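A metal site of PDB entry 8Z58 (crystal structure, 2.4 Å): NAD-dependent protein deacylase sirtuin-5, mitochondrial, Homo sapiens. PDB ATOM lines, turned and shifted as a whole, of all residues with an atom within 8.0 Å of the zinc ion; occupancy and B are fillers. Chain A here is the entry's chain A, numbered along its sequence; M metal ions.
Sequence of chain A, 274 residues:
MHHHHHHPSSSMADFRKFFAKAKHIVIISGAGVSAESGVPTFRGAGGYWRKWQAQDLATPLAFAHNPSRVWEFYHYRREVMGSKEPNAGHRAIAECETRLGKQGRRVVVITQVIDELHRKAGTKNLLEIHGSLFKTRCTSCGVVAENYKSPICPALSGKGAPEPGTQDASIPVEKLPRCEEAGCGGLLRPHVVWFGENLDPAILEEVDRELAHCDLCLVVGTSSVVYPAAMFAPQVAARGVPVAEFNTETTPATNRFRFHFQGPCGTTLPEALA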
ATOM      1  N   ARG A 137     -17.345  -5.746  22.104  1.00  0.00           N
ATOM      2  CA  ARG A 137     -18.641  -5.126  22.269  1.00  0.00           C
ATOM      3  C   ARG A 137     -18.488  -3.623  22.102  1.00  0.00           C
ATOM      4  O   ARG A 137     -17.509  -3.041  22.587  1.00  0.00           O
ATOM      5  CB  ARG A 137     -19.235  -5.455  23.654  1.00  0.00           C
ATOM      6  CG  ARG A 137     -20.704  -5.090  23.802  1.00  0.00           C
ATOM      7  CD  ARG A 137     -21.340  -5.760  25.019  1.00  0.00           C
ATOM      8  NE  ARG A 137     -21.108  -5.046  26.266  1.00  0.00           N
ATOM      9  CZ  ARG A 137     -20.510  -5.551  27.345  1.00  0.00           C
ATOM     10  NH1 ARG A 137     -20.078  -6.807  27.360  1.00  0.00           N
ATOM     11  NH2 ARG A 137     -20.375  -4.807  28.430  1.00  0.00           N
ATOM     12  N   CYS A 138     -19.436  -3.001  21.410  1.00  0.00           N
ATOM     13  CA  CYS A 138     -19.395  -1.561  21.145  1.00  0.00           C
ATOM     14  C   CYS A 138     -20.062  -0.804  22.283  1.00  0.00           C
ATOM     15  O   CYS A 138     -21.245  -1.027  22.581  1.00  0.00           O
ATOM     16  CB  CYS A 138     -20.103  -1.240  19.825  1.00  0.00           C
ATOM     17  SG  CYS A 138     -20.002   0.516  19.370  1.00  0.00           S
ATOM     18  N   THR A 139     -19.305   0.109  22.899  1.00  0.00           N
ATOM     19  CA  THR A 139     -19.834   0.898  23.998  1.00  0.00           C
ATOM     20  C   THR A 139     -20.901   1.894  23.572  1.00  0.00           C
ATOM     21  O   THR A 139     -21.534   2.517  24.437  1.00  0.00           O
ATOM     22  CB  THR A 139     -18.700   1.637  24.725  1.00  0.00           C
ATOM     23  OG1 THR A 139     -18.015   2.493  23.802  1.00  0.00           O
ATOM     24  CG2 THR A 139     -17.721   0.629  25.312  1.00  0.00           C
ATOM     25  N   SER A 140     -21.139   2.061  22.272  1.00  0.00           N
ATOM     26  CA  SER A 140     -22.187   2.951  21.778  1.00  0.00           C
ATOM     27  C   SER A 140     -23.443   2.198  21.361  1.00  0.00           C
ATOM     28  O   SER A 140     -24.532   2.502  21.849  1.00  0.00           O
ATOM     29  CB  SER A 140     -21.659   3.804  20.620  1.00  0.00           C
ATOM     30  OG  SER A 140     -20.660   4.712  21.066  1.00  0.00           O
ATOM     31  N   CYS A 141     -23.320   1.233  20.453  1.00  0.00           N
ATOM     32  CA  CYS A 141     -24.478   0.574  19.884  1.00  0.00           C
ATOM     33  C   CYS A 141     -24.726  -0.825  20.448  1.00  0.00           C
ATOM     34  O   CYS A 141     -25.777  -1.396  20.176  1.00  0.00           O
ATOM     35  CB  CYS A 141     -24.390   0.526  18.353  1.00  0.00           C
ATOM     36  SG  CYS A 141     -23.214  -0.687  17.649  1.00  0.00           S
ATOM     37  N   GLY A 142     -23.778  -1.377  21.196  1.00  0.00           N
ATOM     38  CA  GLY A 142     -23.972  -2.645  21.882  1.00  0.00           C
ATOM     39  C   GLY A 142     -23.766  -3.908  21.058  1.00  0.00           C
ATOM     40  O   GLY A 142     -23.925  -5.011  21.603  1.00  0.00           O
ATOM     41  N   VAL A 143     -23.392  -3.795  19.787  1.00  0.00           N
ATOM     42  CA  VAL A 143     -23.250  -4.985  18.941  1.00  0.00           C
ATOM     43  C   VAL A 143     -22.002  -5.761  19.349  1.00  0.00           C
ATOM     44  O   VAL A 143     -20.967  -5.183  19.681  1.00  0.00           O
ATOM     45  CB  VAL A 143     -23.275  -4.619  17.446  1.00  0.00           C
ATOM     46  CG1 VAL A 143     -21.991  -3.963  17.029  1.00  0.00           C
ATOM     47  CG2 VAL A 143     -23.530  -5.862  16.601  1.00  0.00           C
ATOM     48  N   VAL A 144     -22.114  -7.088  19.337  1.00  0.00           N
ATOM     49  CA  VAL A 144     -21.030  -7.983  19.702  1.00  0.00           C
ATOM     50  C   VAL A 144     -20.501  -8.629  18.434  1.00  0.00           C
ATOM     51  O   VAL A 144     -21.271  -8.923  17.517  1.00  0.00           O
ATOM     52  CB  VAL A 144     -21.513  -9.045  20.708  1.00  0.00           C
ATOM     53  CG1 VAL A 144     -20.331  -9.845  21.259  1.00  0.00           C
ATOM     54  CG2 VAL A 144     -22.303  -8.404  21.821  1.00  0.00           C
ATOM     55  N   ARG A 178     -12.343   0.374  17.254  1.00  0.00           N
ATOM     56  CA  ARG A 178     -13.583   1.111  17.027  1.00  0.00           C
ATOM     57  C   ARG A 178     -14.625   0.219  16.372  1.00  0.00           C
ATOM     58  O   ARG A 178     -14.297  -0.760  15.702  1.00  0.00           O
ATOM     59  CB  ARG A 178     -13.346   2.333  16.131  1.00  0.00           C
ATOM     60  CG  ARG A 178     -12.179   3.224  16.519  1.00  0.00           C
ATOM     61  CD  ARG A 178     -12.389   3.880  17.868  1.00  0.00           C
ATOM     62  NE  ARG A 178     -13.705   4.515  17.974  1.00  0.00           N
ATOM     63  CZ  ARG A 178     -14.065   5.327  18.958  1.00  0.00           C
ATOM     64  NH1 ARG A 178     -13.198   5.617  19.922  1.00  0.00           N
ATOM     65  NH2 ARG A 178     -15.283   5.845  18.981  1.00  0.00           N
ATOM     66  N   CYS A 179     -15.888   0.590  16.556  1.00  0.00           N
ATOM     67  CA  CYS A 179     -16.984  -0.173  15.969  1.00  0.00           C
ATOM     68  C   CYS A 179     -17.009   0.030  14.465  1.00  0.00           C
ATOM     69  O   CYS A 179     -17.070   1.158  13.970  1.00  0.00           O
ATOM     70  CB  CYS A 179     -18.306   0.279  16.582  1.00  0.00           C
ATOM     71  SG  CYS A 179     -19.719  -0.750  16.095  1.00  0.00           S
ATOM     72  N   GLU A 180     -16.986  -1.075  13.720  1.00  0.00           N
ATOM     73  CA  GLU A 180     -17.013  -1.029  12.261  1.00  0.00           C
ATOM     74  C   GLU A 180     -18.428  -1.029  11.697  1.00  0.00           C
ATOM     75  O   GLU A 180     -18.589  -0.969  10.472  1.00  0.00           O
ATOM     76  CB  GLU A 180     -16.173  -2.161  11.661  1.00  0.00           C
ATOM     77  CG  GLU A 180     -14.662  -1.981  11.905  1.00  0.00           C
ATOM     78  CD  GLU A 180     -13.817  -3.047  11.233  1.00  0.00           C
ATOM     79  OE1 GLU A 180     -12.737  -3.374  11.759  1.00  0.00           O
ATOM     80  OE2 GLU A 180     -14.234  -3.545  10.163  1.00  0.00           O
ATOM     81  N   GLU A 181     -19.442  -1.078  12.550  1.00  0.00           N
ATOM     82  CA  GLU A 181     -20.816  -0.922  12.075  1.00  0.00           C
ATOM     83  C   GLU A 181     -20.975   0.459  11.449  1.00  0.00           C
ATOM     84  O   GLU A 181     -20.545   1.468  12.012  1.00  0.00           O
ATOM     85  CB  GLU A 181     -21.785  -1.089  13.249  1.00  0.00           C
ATOM     86  CG  GLU A 181     -23.085  -1.793  12.899  1.00  0.00           C
ATOM     87  CD  GLU A 181     -22.883  -3.228  12.476  1.00  0.00           C
ATOM     88  OE1 GLU A 181     -23.583  -3.684  11.545  1.00  0.00           O
ATOM     89  OE2 GLU A 181     -22.019  -3.907  13.059  1.00  0.00           O
ATOM     90  N   ALA A 182     -21.563   0.491  10.251  1.00  0.00           N
ATOM     91  CA  ALA A 182     -21.681   1.737   9.517  1.00  0.00           C
ATOM     92  C   ALA A 182     -22.510   2.739  10.303  1.00  0.00           C
ATOM     93  O   ALA A 182     -23.615   2.440  10.758  1.00  0.00           O
ATOM     94  CB  ALA A 182     -22.325   1.476   8.155  1.00  0.00           C
ATOM     95  N   GLY A 183     -21.965   3.946  10.469  1.00  0.00           N
ATOM     96  CA  GLY A 183     -22.648   5.014  11.171  1.00  0.00           C
ATOM     97  C   GLY A 183     -22.343   5.122  12.646  1.00  0.00           C
ATOM     98  O   GLY A 183     -22.697   6.129  13.256  1.00  0.00           O
ATOM     99  N   CYS A 184     -21.690   4.124  13.241  1.00  0.00           N
ATOM    100  CA  CYS A 184     -21.423   4.138  14.672  1.00  0.00           C
ATOM    101  C   CYS A 184     -19.995   4.574  14.998  1.00  0.00           C
ATOM    102  O   CYS A 184     -19.782   5.641  15.575  1.00  0.00           O
ATOM    103  CB  CYS A 184     -21.718   2.757  15.265  1.00  0.00           C
ATOM    104  SG  CYS A 184     -21.375   2.629  17.026  1.00  0.00           S
ATOM    105  N   GLY A 185     -19.008   3.775  14.583  1.00  0.00           N
ATOM    106  CA  GLY A 185     -17.623   4.060  14.907  1.00  0.00           C
ATOM    107  C   GLY A 185     -17.331   4.240  16.380  1.00  0.00           C
ATOM    108  O   GLY A 185     -16.293   4.811  16.733  1.00  0.00           O
ATOM    109  N   GLY A 186     -18.219   3.758  17.242  1.00  0.00           N
ATOM    110  CA  GLY A 186     -18.028   3.909  18.671  1.00  0.00           C
ATOM    111  C   GLY A 186     -16.843   3.118  19.192  1.00  0.00           C
ATOM    112  O   GLY A 186     -16.242   2.284  18.503  1.00  0.00           O
ATOM    113  N   LEU A 187     -16.483   3.402  20.439  1.00  0.00           N
ATOM    114  CA  LEU A 187     -15.349   2.749  21.066  1.00  0.00           C
ATOM    115  C   LEU A 187     -15.721   1.337  21.493  1.00  0.00           C
ATOM    116  O   LEU A 187     -16.730   1.138  22.188  1.00  0.00           O
ATOM    117  CB  LEU A 187     -14.869   3.543  22.281  1.00  0.00           C
ATOM    118  CG  LEU A 187     -13.731   2.874  23.058  1.00  0.00           C
ATOM    119  CD1 LEU A 187     -12.474   2.746  22.189  1.00  0.00           C
ATOM    120  CD2 LEU A 187     -13.430   3.610  24.368  1.00  0.00           C
ATOM    121  N   LEU A 188     -14.914   0.372  21.097  1.00  0.00           N
ATOM    122  CA  LEU A 188     -15.134  -1.018  21.467  1.00  0.00           C
ATOM    123  C   LEU A 188     -14.490  -1.314  22.810  1.00  0.00           C
ATOM    124  O   LEU A 188     -13.484  -0.719  23.189  1.00  0.00           O
ATOM    125  CB  LEU A 188     -14.527  -1.951  20.424  1.00  0.00           C
ATOM    126  CG  LEU A 188     -15.098  -1.930  19.002  1.00  0.00           C
ATOM    127  CD1 LEU A 188     -14.434  -3.012  18.159  1.00  0.00           C
ATOM    128  CD2 LEU A 188     -16.600  -2.127  19.009  1.00  0.00           C
HETATM  129 ZN    ZN M   1     -21.155   0.419  17.452  1.00  0.00          ZN
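Of the 19 residues printed, 4 come within 4 Å of the zinc ion.
The nearest printed residue that does not touch the zinc ion is Gly 186 (4.5 Å).
The side-chain sulfur (SG) of Cys 141 lies close to the backbone NH (N) of Val 143, at 3.8 Å.
SG of Cys 179 lies close to N of Glu 181, 3.6 Å away.
The backbone carbonyl oxygen (O) of Cys 179 sits close to the backbone NH (N) of Gly 185.
O of Gly 186 is in hydrogen-bond range of N of Cys 179 (2.6 Å).
The backbone NH of Gly 186 lies close to the side-chain sulfur of Cys 184 (3.4 Å).
SG of Cys 138 lies close to N of Ser 140 (3.5 Å).
N of Cys 138 sits at hydrogen-bond distance from O of Val 143 (3.2 Å).
The zinc ion is bound by the side-chain sulfur of Cys 138 (2.2 Å), the side-chain sulfur of Cys 184 (2.3 Å), the side-chain sulfur of Cys 179 (2.3 Å) and the side-chain sulfur of Cys 141 (2.3 Å).
The zinc ion has four donor atoms within binding distance.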
